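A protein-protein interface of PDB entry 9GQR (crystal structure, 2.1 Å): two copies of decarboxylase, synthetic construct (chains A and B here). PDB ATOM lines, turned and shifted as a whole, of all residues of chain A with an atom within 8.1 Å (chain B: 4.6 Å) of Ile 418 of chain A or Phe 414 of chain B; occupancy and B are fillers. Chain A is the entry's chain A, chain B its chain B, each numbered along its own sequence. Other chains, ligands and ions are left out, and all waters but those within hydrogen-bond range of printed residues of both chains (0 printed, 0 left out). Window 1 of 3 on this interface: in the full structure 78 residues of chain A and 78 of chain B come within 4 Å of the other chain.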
ATOM      1  N   PRO A 355      25.413 -12.255  12.053  1.00  0.00           N
ATOM      2  CA  PRO A 355      25.781 -13.648  12.337  1.00  0.00           C
ATOM      3  C   PRO A 355      26.716 -14.197  11.271  1.00  0.00           C
ATOM      4  O   PRO A 355      26.434 -14.118  10.073  1.00  0.00           O
ATOM      5  CB  PRO A 355      24.433 -14.377  12.342  1.00  0.00           C
ATOM      6  CG  PRO A 355      23.437 -13.317  12.691  1.00  0.00           C
ATOM      7  CD  PRO A 355      23.952 -12.060  12.043  1.00  0.00           C
ATOM      8  N   GLU A 357      27.440 -17.223  10.533  1.00  0.00           N
ATOM      9  CA  GLU A 357      26.879 -18.351   9.799  1.00  0.00           C
ATOM     10  C   GLU A 357      26.101 -17.909   8.566  1.00  0.00           C
ATOM     11  O   GLU A 357      25.932 -18.703   7.636  1.00  0.00           O
ATOM     12  CB  GLU A 357      25.974 -19.182  10.715  1.00  0.00           C
ATOM     13  CG  GLU A 357      26.709 -19.937  11.819  1.00  0.00           C
ATOM     14  CD  GLU A 357      27.109 -19.050  12.986  1.00  0.00           C
ATOM     15  OE1 GLU A 357      26.783 -17.845  12.972  1.00  0.00           O
ATOM     16  OE2 GLU A 357      27.751 -19.560  13.927  1.00  0.00           O
ATOM     17  N   TRP A 362      23.286 -11.316   6.800  1.00  0.00           N
ATOM     18  CA  TRP A 362      22.222 -10.994   7.739  1.00  0.00           C
ATOM     19  C   TRP A 362      22.689  -9.916   8.705  1.00  0.00           C
ATOM     20  O   TRP A 362      23.861  -9.882   9.094  1.00  0.00           O
ATOM     21  CB  TRP A 362      21.789 -12.230   8.531  1.00  0.00           C
ATOM     22  CG  TRP A 362      20.979 -13.217   7.752  1.00  0.00           C
ATOM     23  CD1 TRP A 362      20.719 -13.194   6.412  1.00  0.00           C
ATOM     24  CD2 TRP A 362      20.317 -14.376   8.271  1.00  0.00           C
ATOM     25  NE1 TRP A 362      19.937 -14.271   6.065  1.00  0.00           N
ATOM     26  CE2 TRP A 362      19.676 -15.011   7.188  1.00  0.00           C
ATOM     27  CE3 TRP A 362      20.206 -14.940   9.546  1.00  0.00           C
ATOM     28  CZ2 TRP A 362      18.932 -16.182   7.343  1.00  0.00           C
ATOM     29  CZ3 TRP A 362      19.468 -16.100   9.698  1.00  0.00           C
ATOM     30  CH2 TRP A 362      18.841 -16.709   8.603  1.00  0.00           C
ATOM     31  N   ILE A 403      17.122  -8.800  10.365  1.00  0.00           N
ATOM     32  CA  ILE A 403      16.305  -9.605  11.266  1.00  0.00           C
ATOM     33  C   ILE A 403      15.986  -8.775  12.500  1.00  0.00           C
ATOM     34  O   ILE A 403      16.895  -8.246  13.152  1.00  0.00           O
ATOM     35  CB  ILE A 403      17.016 -10.911  11.661  1.00  0.00           C
ATOM     36  CG1 ILE A 403      17.441 -11.676  10.412  1.00  0.00           C
ATOM     37  CG2 ILE A 403      16.101 -11.772  12.516  1.00  0.00           C
ATOM     38  CD1 ILE A 403      16.306 -11.860   9.418  1.00  0.00           C
ATOM     39  N   VAL A 405      14.533  -8.997  16.206  1.00  0.00           N
ATOM     40  CA  VAL A 405      14.241  -9.918  17.293  1.00  0.00           C
ATOM     41  C   VAL A 405      14.061  -9.130  18.584  1.00  0.00           C
ATOM     42  O   VAL A 405      14.514  -7.989  18.717  1.00  0.00           O
ATOM     43  CB  VAL A 405      15.339 -10.991  17.471  1.00  0.00           C
ATOM     44  CG1 VAL A 405      15.477 -11.830  16.212  1.00  0.00           C
ATOM     45  CG2 VAL A 405      16.660 -10.339  17.842  1.00  0.00           C
ATOM     46  N   ILE A 409      16.769 -12.520  22.944  1.00  0.00           N
ATOM     47  CA  ILE A 409      17.589 -13.269  21.998  1.00  0.00           C
ATOM     48  C   ILE A 409      19.010 -12.723  22.040  1.00  0.00           C
ATOM     49  O   ILE A 409      19.243 -11.555  21.704  1.00  0.00           O
ATOM     50  CB  ILE A 409      17.025 -13.193  20.570  1.00  0.00           C
ATOM     51  CG1 ILE A 409      15.671 -13.901  20.489  1.00  0.00           C
ATOM     52  CG2 ILE A 409      18.020 -13.780  19.576  1.00  0.00           C
ATOM     53  CD1 ILE A 409      15.721 -15.351  20.909  1.00  0.00           C
ATOM     54  N   ASP A 410      19.960 -13.568  22.434  1.00  0.00           N
ATOM     55  CA  ASP A 410      21.379 -13.221  22.350  1.00  0.00           C
ATOM     56  C   ASP A 410      21.791 -13.337  20.888  1.00  0.00           C
ATOM     57  O   ASP A 410      22.057 -14.434  20.390  1.00  0.00           O
ATOM     58  CB  ASP A 410      22.212 -14.134  23.243  1.00  0.00           C
ATOM     59  CG  ASP A 410      23.696 -13.809  23.198  1.00  0.00           C
ATOM     60  OD1 ASP A 410      24.073 -12.758  22.635  1.00  0.00           O
ATOM     61  OD2 ASP A 410      24.487 -14.618  23.728  1.00  0.00           O
ATOM     62  N   ILE A 411      21.847 -12.198  20.192  1.00  0.00           N
ATOM     63  CA  ILE A 411      22.098 -12.213  18.755  1.00  0.00           C
ATOM     64  C   ILE A 411      23.521 -12.640  18.418  1.00  0.00           C
ATOM     65  O   ILE A 411      23.791 -13.027  17.274  1.00  0.00           O
ATOM     66  CB  ILE A 411      21.790 -10.837  18.139  1.00  0.00           C
ATOM     67  CG1 ILE A 411      22.663  -9.754  18.776  1.00  0.00           C
ATOM     68  CG2 ILE A 411      20.316 -10.503  18.299  1.00  0.00           C
ATOM     69  CD1 ILE A 411      22.476  -8.385  18.157  1.00  0.00           C
ATOM     70  N   ASP A 413      24.795 -15.270  19.534  1.00  0.00           N
ATOM     71  CA  ASP A 413      24.741 -16.721  19.677  1.00  0.00           C
ATOM     72  C   ASP A 413      23.803 -17.242  18.596  1.00  0.00           C
ATOM     73  O   ASP A 413      22.583 -17.077  18.699  1.00  0.00           O
ATOM     74  CB  ASP A 413      24.261 -17.102  21.079  1.00  0.00           C
ATOM     75  CG  ASP A 413      24.221 -18.603  21.313  1.00  0.00           C
ATOM     76  OD1 ASP A 413      24.465 -19.383  20.367  1.00  0.00           O
ATOM     77  OD2 ASP A 413      23.946 -19.002  22.468  1.00  0.00           O
ATOM     78  N   PHE A 414      24.368 -17.873  17.563  1.00  0.00           N
ATOM     79  CA  PHE A 414      23.564 -18.230  16.400  1.00  0.00           C
ATOM     80  C   PHE A 414      22.527 -19.304  16.701  1.00  0.00           C
ATOM     81  O   PHE A 414      21.523 -19.388  15.986  1.00  0.00           O
ATOM     82  CB  PHE A 414      24.450 -18.692  15.245  1.00  0.00           C
ATOM     83  CG  PHE A 414      23.709 -18.828  13.947  1.00  0.00           C
ATOM     84  CD1 PHE A 414      23.214 -17.706  13.302  1.00  0.00           C
ATOM     85  CD2 PHE A 414      23.489 -20.071  13.382  1.00  0.00           C
ATOM     86  CE1 PHE A 414      22.520 -17.821  12.111  1.00  0.00           C
ATOM     87  CE2 PHE A 414      22.795 -20.194  12.189  1.00  0.00           C
ATOM     88  CZ  PHE A 414      22.310 -19.068  11.554  1.00  0.00           C
ATOM     89  N   ARG A 415      22.749 -20.134  17.723  1.00  0.00           N
ATOM     90  CA  ARG A 415      21.719 -21.087  18.126  1.00  0.00           C
ATOM     91  C   ARG A 415      20.432 -20.364  18.497  1.00  0.00           C
ATOM     92  O   ARG A 415      19.332 -20.835  18.186  1.00  0.00           O
ATOM     93  CB  ARG A 415      22.210 -21.934  19.300  1.00  0.00           C
ATOM     94  CG  ARG A 415      23.444 -22.767  19.004  1.00  0.00           C
ATOM     95  CD  ARG A 415      24.021 -23.337  20.286  1.00  0.00           C
ATOM     96  NE  ARG A 415      24.365 -22.278  21.228  1.00  0.00           N
ATOM     97  CZ  ARG A 415      24.814 -22.483  22.459  1.00  0.00           C
ATOM     98  NH1 ARG A 415      24.982 -23.704  22.938  1.00  0.00           N
ATOM     99  NH2 ARG A 415      25.102 -21.436  23.227  1.00  0.00           N
ATOM    100  N   LYS A 416      20.554 -19.212  19.154  1.00  0.00           N
ATOM    101  CA  LYS A 416      19.385 -18.427  19.529  1.00  0.00           C
ATOM    102  C   LYS A 416      18.830 -17.642  18.348  1.00  0.00           C
ATOM    103  O   LYS A 416      17.615 -17.430  18.262  1.00  0.00           O
ATOM    104  CB  LYS A 416      19.737 -17.471  20.669  1.00  0.00           C
ATOM    105  CG  LYS A 416      20.534 -18.107  21.799  1.00  0.00           C
ATOM    106  CD  LYS A 416      19.733 -19.187  22.506  1.00  0.00           C
ATOM    107  CE  LYS A 416      20.505 -19.767  23.685  1.00  0.00           C
ATOM    108  NZ  LYS A 416      21.735 -20.495  23.256  1.00  0.00           N
ATOM    109  N   VAL A 417      19.701 -17.207  17.435  1.00  0.00           N
ATOM    110  CA  VAL A 417      19.254 -16.434  16.280  1.00  0.00           C
ATOM    111  C   VAL A 417      18.450 -17.309  15.329  1.00  0.00           C
ATOM    112  O   VAL A 417      17.366 -16.926  14.875  1.00  0.00           O
ATOM    113  CB  VAL A 417      20.457 -15.789  15.567  1.00  0.00           C
ATOM    114  CG1 VAL A 417      20.019 -15.143  14.255  1.00  0.00           C
ATOM    115  CG2 VAL A 417      21.116 -14.764  16.466  1.00  0.00           C
ATOM    116  N   ILE A 418      18.972 -18.496  15.005  1.00  0.00           N
ATOM    117  CA  ILE A 418      18.276 -19.369  14.067  1.00  0.00           C
ATOM    118  C   ILE A 418      16.973 -19.876  14.671  1.00  0.00           C
ATOM    119  O   ILE A 418      16.013 -20.162  13.944  1.00  0.00           O
ATOM    120  CB  ILE A 418      19.194 -20.528  13.627  1.00  0.00           C
ATOM    121  CG1 ILE A 418      18.617 -21.229  12.395  1.00  0.00           C
ATOM    122  CG2 ILE A 418      19.398 -21.523  14.756  1.00  0.00           C
ATOM    123  CD1 ILE A 418      18.516 -20.324  11.175  1.00  0.00           C
ATOM    124  N   TRP A 419      16.908 -19.985  16.000  1.00  0.00           N
ATOM    125  CA  TRP A 419      15.669 -20.405  16.648  1.00  0.00           C
ATOM    126  C   TRP A 419      14.598 -19.332  16.516  1.00  0.00           C
ATOM    127  O   TRP A 419      13.480 -19.606  16.063  1.00  0.00           O
ATOM    128  CB  TRP A 419      15.935 -20.733  18.118  1.00  0.00           C
ATOM    129  CG  TRP A 419      14.698 -20.985  18.920  1.00  0.00           C
ATOM    130  CD1 TRP A 419      13.748 -21.939  18.689  1.00  0.00           C
ATOM    131  CD2 TRP A 419      14.284 -20.286  20.100  1.00  0.00           C
ATOM    132  NE1 TRP A 419      12.764 -21.868  19.644  1.00  0.00           N
ATOM    133  CE2 TRP A 419      13.070 -20.863  20.524  1.00  0.00           C
ATOM    134  CE3 TRP A 419      14.821 -19.224  20.836  1.00  0.00           C
ATOM    135  CZ2 TRP A 419      12.384 -20.414  21.651  1.00  0.00           C
ATOM    136  CZ3 TRP A 419      14.137 -18.781  21.956  1.00  0.00           C
ATOM    137  CH2 TRP A 419      12.932 -19.374  22.350  1.00  0.00           C
ATOM    138  N   ALA A 420      14.929 -18.097  16.901  1.00  0.00           N
ATOM    139  CA  ALA A 420      13.979 -16.998  16.760  1.00  0.00           C
ATOM    140  C   ALA A 420      13.623 -16.748  15.302  1.00  0.00           C
ATOM    141  O   ALA A 420      12.486 -16.376  14.998  1.00  0.00           O
ATOM    142  CB  ALA A 420      14.545 -15.728  17.396  1.00  0.00           C
ATOM    143  N   TYR A 421      14.572 -16.954  14.386  1.00  0.00           N
ATOM    144  CA  TYR A 421      14.289 -16.731  12.972  1.00  0.00           C
ATOM    145  C   TYR A 421      13.252 -17.719  12.454  1.00  0.00           C
ATOM    146  O   TYR A 421      12.257 -17.329  11.831  1.00  0.00           O
ATOM    147  CB  TYR A 421      15.577 -16.831  12.153  1.00  0.00           C
ATOM    148  CG  TYR A 421      15.379 -16.569  10.679  1.00  0.00           C
ATOM    149  CD1 TYR A 421      15.292 -15.269  10.195  1.00  0.00           C
ATOM    150  CD2 TYR A 421      15.276 -17.620   9.771  1.00  0.00           C
ATOM    151  CE1 TYR A 421      15.109 -15.018   8.851  1.00  0.00           C
ATOM    152  CE2 TYR A 421      15.093 -17.380   8.422  1.00  0.00           C
ATOM    153  CZ  TYR A 421      15.009 -16.075   7.970  1.00  0.00           C
ATOM    154  OH  TYR A 421      14.829 -15.813   6.630  1.00  0.00           O
ATOM    155  N   THR A 422      13.467 -19.012  12.708  1.00  0.00           N
ATOM    156  CA  THR A 422      12.613 -20.031  12.108  1.00  0.00           C
ATOM    157  C   THR A 422      11.240 -20.098  12.767  1.00  0.00           C
ATOM    158  O   THR A 422      10.268 -20.503  12.120  1.00  0.00           O
ATOM    159  CB  THR A 422      13.297 -21.397  12.180  1.00  0.00           C
ATOM    160  OG1 THR A 422      13.658 -21.683  13.538  1.00  0.00           O
ATOM    161  CG2 THR A 422      14.549 -21.414  11.312  1.00  0.00           C
ATOM    162  N   THR A 423      11.133 -19.706  14.038  1.00  0.00           N
ATOM    163  CA  THR A 423       9.900 -19.896  14.791  1.00  0.00           C
ATOM    164  C   THR A 423       9.094 -18.624  15.016  1.00  0.00           C
ATOM    165  O   THR A 423       7.953 -18.720  15.482  1.00  0.00           O
ATOM    166  CB  THR A 423      10.199 -20.537  16.157  1.00  0.00           C
ATOM    167  OG1 THR A 423      10.966 -19.634  16.965  1.00  0.00           O
ATOM    168  CG2 THR A 423      10.978 -21.833  15.987  1.00  0.00           C
ATOM    169  N   ARG A 424       9.631 -17.444  14.699  1.00  0.00           N
ATOM    170  CA  ARG A 424       8.945 -16.197  15.022  1.00  0.00           C
ATOM    171  C   ARG A 424       8.626 -15.331  13.808  1.00  0.00           C
ATOM    172  O   ARG A 424       8.172 -14.193  13.983  1.00  0.00           O
ATOM    173  CB  ARG A 424       9.765 -15.378  16.025  1.00  0.00           C
ATOM    174  CG  ARG A 424      10.090 -16.111  17.312  1.00  0.00           C
ATOM    175  CD  ARG A 424      10.824 -15.211  18.291  1.00  0.00           C
ATOM    176  NE  ARG A 424      11.330 -15.955  19.439  1.00  0.00           N
ATOM    177  CZ  ARG A 424      11.900 -15.398  20.500  1.00  0.00           C
ATOM    178  NH1 ARG A 424      12.049 -14.089  20.597  1.00  0.00           N
ATOM    179  NH2 ARG A 424      12.326 -16.178  21.489  1.00  0.00           N
ATOM    180  N   HIS A 425       8.846 -15.818  12.591  1.00  0.00           N
ATOM    181  CA  HIS A 425       8.483 -15.061  11.402  1.00  0.00           C
ATOM    182  C   HIS A 425       7.716 -15.956  10.442  1.00  0.00           C
ATOM    183  O   HIS A 425       8.086 -17.114  10.221  1.00  0.00           O
ATOM    184  CB  HIS A 425       9.723 -14.456  10.710  1.00  0.00           C
ATOM    185  CG  HIS A 425      10.225 -15.249   9.542  1.00  0.00           C
ATOM    186  ND1 HIS A 425      11.179 -16.237   9.667  1.00  0.00           N
ATOM    187  CD2 HIS A 425       9.921 -15.184   8.224  1.00  0.00           C
ATOM    188  CE1 HIS A 425      11.432 -16.754   8.477  1.00  0.00           C
ATOM    189  NE2 HIS A 425      10.683 -16.132   7.585  1.00  0.00           N
ATOM    190  N   CYS A 464      10.838 -10.859  13.174  1.00  0.00           N
ATOM    191  CA  CYS A 464      10.783 -12.043  14.020  1.00  0.00           C
ATOM    192  C   CYS A 464      10.330 -11.690  15.434  1.00  0.00           C
ATOM    193  O   CYS A 464      10.722 -12.341  16.406  1.00  0.00           O
ATOM    194  CB  CYS A 464      12.137 -12.750  14.043  1.00  0.00           C
ATOM    195  SG  CYS A 464      12.711 -13.255  12.408  1.00  0.00           S
ATOM    196  N   PRO B 355      16.053 -30.076   8.919  1.00  0.00           N
ATOM    197  CA  PRO B 355      17.105 -29.603   9.829  1.00  0.00           C
ATOM    198  C   PRO B 355      16.554 -29.337  11.222  1.00  0.00           C
ATOM    199  O   PRO B 355      15.571 -28.611  11.394  1.00  0.00           O
ATOM    200  CB  PRO B 355      17.600 -28.318   9.157  1.00  0.00           C
ATOM    201  CG  PRO B 355      17.277 -28.507   7.710  1.00  0.00           C
ATOM    202  CD  PRO B 355      15.987 -29.276   7.683  1.00  0.00           C
ATOM    203  N   GLU B 357      17.836 -27.620  13.598  1.00  0.00           N
ATOM    204  CA  GLU B 357      17.996 -26.228  14.001  1.00  0.00           C
ATOM    205  C   GLU B 357      16.814 -25.365  13.578  1.00  0.00           C
ATOM    206  O   GLU B 357      16.634 -24.270  14.121  1.00  0.00           O
ATOM    207  CB  GLU B 357      19.294 -25.656  13.423  1.00  0.00           C
ATOM    208  CG  GLU B 357      20.573 -26.217  14.043  1.00  0.00           C
ATOM    209  CD  GLU B 357      20.959 -27.581  13.493  1.00  0.00           C
ATOM    210  OE1 GLU B 357      20.174 -28.157  12.711  1.00  0.00           O
ATOM    211  OE2 GLU B 357      22.054 -28.075  13.837  1.00  0.00           O
ATOM    212  N   TRP B 362      11.485 -26.603   8.689  1.00  0.00           N
ATOM    213  CA  TRP B 362      12.102 -26.606   7.370  1.00  0.00           C
ATOM    214  C   TRP B 362      12.169 -28.023   6.821  1.00  0.00           C
ATOM    215  O   TRP B 362      12.414 -28.979   7.563  1.00  0.00           O
ATOM    216  CB  TRP B 362      13.515 -26.021   7.419  1.00  0.00           C
ATOM    217  CG  TRP B 362      13.574 -24.529   7.550  1.00  0.00           C
ATOM    218  CD1 TRP B 362      12.526 -23.673   7.732  1.00  0.00           C
ATOM    219  CD2 TRP B 362      14.753 -23.715   7.506  1.00  0.00           C
ATOM    220  NE1 TRP B 362      12.980 -22.376   7.804  1.00  0.00           N
ATOM    221  CE2 TRP B 362      14.345 -22.376   7.668  1.00  0.00           C
ATOM    222  CE3 TRP B 362      16.116 -23.990   7.349  1.00  0.00           C
ATOM    223  CZ2 TRP B 362      15.249 -21.315   7.672  1.00  0.00           C
ATOM    224  CZ3 TRP B 362      17.011 -22.936   7.348  1.00  0.00           C
ATOM    225  CH2 TRP B 362      16.576 -21.614   7.511  1.00  0.00           C
ATOM    226  N   PHE B 412      22.084 -33.036   5.757  1.00  0.00           N
ATOM    227  CA  PHE B 412      22.154 -33.516   7.132  1.00  0.00           C
ATOM    228  C   PHE B 412      23.187 -32.764   7.961  1.00  0.00           C
ATOM    229  O   PHE B 412      23.337 -33.054   9.153  1.00  0.00           O
ATOM    230  CB  PHE B 412      22.463 -35.016   7.153  1.00  0.00           C
ATOM    231  CG  PHE B 412      21.450 -35.853   6.426  1.00  0.00           C
ATOM    232  CD1 PHE B 412      20.264 -36.218   7.044  1.00  0.00           C
ATOM    233  CD2 PHE B 412      21.680 -36.278   5.126  1.00  0.00           C
ATOM    234  CE1 PHE B 412      19.326 -36.990   6.382  1.00  0.00           C
ATOM    235  CE2 PHE B 412      20.745 -37.052   4.458  1.00  0.00           C
ATOM    236  CZ  PHE B 412      19.566 -37.408   5.088  1.00  0.00           C
ATOM    237  N   ASP B 413      23.893 -31.812   7.357  1.00  0.00           N
ATOM    238  CA  ASP B 413      24.899 -30.994   8.028  1.00  0.00           C
ATOM    239  C   ASP B 413      24.425 -29.550   7.946  1.00  0.00           C
ATOM    240  O   ASP B 413      24.477 -28.938   6.874  1.00  0.00           O
ATOM    241  CB  ASP B 413      26.270 -31.177   7.373  1.00  0.00           C
ATOM    242  CG  ASP B 413      27.381 -30.437   8.101  1.00  0.00           C
ATOM    243  OD1 ASP B 413      27.090 -29.701   9.068  1.00  0.00           O
ATOM    244  OD2 ASP B 413      28.557 -30.600   7.702  1.00  0.00           O
ATOM    245  N   PHE B 414      23.964 -29.007   9.077  1.00  0.00           N
ATOM    246  CA  PHE B 414      23.307 -27.704   9.047  1.00  0.00           C
ATOM    247  C   PHE B 414      24.259 -26.578   8.675  1.00  0.00           C
ATOM    248  O   PHE B 414      23.800 -25.521   8.224  1.00  0.00           O
ATOM    249  CB  PHE B 414      22.643 -27.398  10.389  1.00  0.00           C
ATOM    250  CG  PHE B 414      21.775 -26.172  10.360  1.00  0.00           C
ATOM    251  CD1 PHE B 414      20.590 -26.170   9.645  1.00  0.00           C
ATOM    252  CD2 PHE B 414      22.148 -25.022  11.035  1.00  0.00           C
ATOM    253  CE1 PHE B 414      19.787 -25.041   9.609  1.00  0.00           C
ATOM    254  CE2 PHE B 414      21.349 -23.891  11.002  1.00  0.00           C
ATOM    255  CZ  PHE B 414      20.169 -23.902  10.289  1.00  0.00           C
ATOM    256  N   ARG B 415      25.566 -26.764   8.868  1.00  0.00           N
ATOM    257  CA  ARG B 415      26.527 -25.750   8.439  1.00  0.00           C
ATOM    258  C   ARG B 415      26.453 -25.533   6.935  1.00  0.00           C
ATOM    259  O   ARG B 415      26.569 -24.400   6.453  1.00  0.00           O
ATOM    260  CB  ARG B 415      27.943 -26.155   8.844  1.00  0.00           C
ATOM    261  CG  ARG B 415      28.172 -26.272  10.334  1.00  0.00           C
ATOM    262  CD  ARG B 415      29.490 -26.972  10.617  1.00  0.00           C
ATOM    263  NE  ARG B 415      29.524 -28.303  10.023  1.00  0.00           N
ATOM    264  CZ  ARG B 415      30.588 -29.094  10.016  1.00  0.00           C
ATOM    265  NH1 ARG B 415      31.733 -28.717  10.560  1.00  0.00           N
ATOM    266  NH2 ARG B 415      30.500 -30.294   9.446  1.00  0.00           N
ATOM    267  N   LYS B 416      26.264 -26.615   6.175  1.00  0.00           N
ATOM    268  CA  LYS B 416      26.107 -26.517   4.732  1.00  0.00           C
ATOM    269  C   LYS B 416      24.720 -26.015   4.354  1.00  0.00           C
ATOM    270  O   LYS B 416      24.575 -25.311   3.348  1.00  0.00           O
ATOM    271  CB  LYS B 416      26.365 -27.880   4.087  1.00  0.00           C
ATOM    272  CG  LYS B 416      27.623 -28.575   4.590  1.00  0.00           C
ATOM    273  CD  LYS B 416      28.873 -27.792   4.222  1.00  0.00           C
ATOM    274  CE  LYS B 416      30.126 -28.420   4.818  1.00  0.00           C
ATOM    275  NZ  LYS B 416      30.217 -28.192   6.288  1.00  0.00           N
ATOM    276  N   VAL B 417      23.701 -26.351   5.148  1.00  0.00           N
ATOM    277  CA  VAL B 417      22.338 -25.923   4.842  1.00  0.00           C
ATOM    278  C   VAL B 417      22.198 -24.416   5.021  1.00  0.00           C
ATOM    279  O   VAL B 417      21.676 -23.717   4.144  1.00  0.00           O
ATOM    280  CB  VAL B 417      21.324 -26.687   5.713  1.00  0.00           C
ATOM    281  CG1 VAL B 417      19.918 -26.168   5.468  1.00  0.00           C
ATOM    282  CG2 VAL B 417      21.401 -28.173   5.428  1.00  0.00           C
ATOM    283  N   ILE B 418      22.655 -23.891   6.161  1.00  0.00           N
ATOM    284  CA  ILE B 418      22.525 -22.458   6.403  1.00  0.00           C
ATOM    285  C   ILE B 418      23.419 -21.670   5.452  1.00  0.00           C
ATOM    286  O   ILE B 418      23.120 -20.516   5.123  1.00  0.00           O
ATOM    287  CB  ILE B 418      22.827 -22.131   7.877  1.00  0.00           C
ATOM    288  CG1 ILE B 418      22.360 -20.715   8.221  1.00  0.00           C
ATOM    289  CG2 ILE B 418      24.309 -22.286   8.177  1.00  0.00           C
ATOM    290  CD1 ILE B 418      20.873 -20.490   7.991  1.00  0.00           C
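Of the 22 printed residues of chain A, 4 touch a printed residue of chain B. Printed residues of chain A that touch a printed residue of chain B: Glu 357, Phe 414, Ile 418 and Thr 422. Hydrophobic or aromatic side chains of chain A within 4 Å of the printed part of chain B: Phe 414 and Ile 418. Of the 10 printed residues of chain B, 4 touch a printed residue of chain A. Among the printed residues, 7 pairs touch across the chains.
Glu 357 of chain A touches Ile 418 of chain B, and with the chains exchanged Ile 418 of chain A touches Glu 357 of chain B. Phe 414 of chain A touches Ile 418 of chain B, and with the chains exchanged Ile 418 of chain A touches Phe 414 of chain B. Ile 418 of chain B touches its own counterpart, Ile 418 of chain A. Positions printed for both chains: 355, 357, 362, 413, 414, 415, 416, 417 and 418. Of the 7 pairs that touch across the chains among the printed residues, 5 have their exchanged pair printed and touching as well.
Ile 418 of chain A touches just these residues of chain B: Glu 357 (3.9 Å), Phe 414 (3.7 Å) and Ile 418 (3.96 Å). Phe 414 of chain B touches one residue of chain A. Of the printed residues of chain B, Thr 422 of chain A touches Glu 357 (3.99 Å) and Trp 362 (3.7 Å). Of the printed residues of chain A, Ile 418 of chain B touches Glu 357 (3.97 Å), Phe 414 (3.7 Å) and Ile 418 (3.96 Å). Of the printed residues of chain A, Glu 357 of chain B touches Ile 418 and Thr 422. Pro 355 of chain A touches none of the printed residues of chain B. The nearest residue of chain B that does not touch Ile 418 of chain A is Trp 362 of chain B (4.3 Å). The nearest residue of chain A that does not touch Phe 414 of chain B is Phe 414 of chain A (4.1 Å). The nearest printed residue of chain A that does not touch Ile 418 of chain B is Trp 362 of chain A (4.3 Å).
Among the printed residues, merely in contact across the chains: Thr 422 of chain A with Trp 362 of chain B (3.7 Å), Phe 414 of chain A with Ile 418 of chain B (3.7 Å), Ile 418 of chain A with Phe 414 of chain B (3.7 Å), Ile 418 of chain A with Glu 357 of chain B (3.9 Å), Ile 418 of chain A with Ile 418 of chain B (3.96 Å), Glu 357 of chain A with Ile 418 of chain B (3.97 Å) and Thr 422 of chain A with Glu 357 of chain B (3.99 Å).
The side-chain hydroxyl of Thr 422 of chain A sits at hydrogen-bond distance from the backbone carbonyl oxygen of Trp 419 of chain A (3.3 Å). The side-chain hydroxyl (OG1) of Thr 422 of chain A is in hydrogen-bond range of the backbone carbonyl oxygen (O) of Ile 418 of chain A (2.8 Å).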
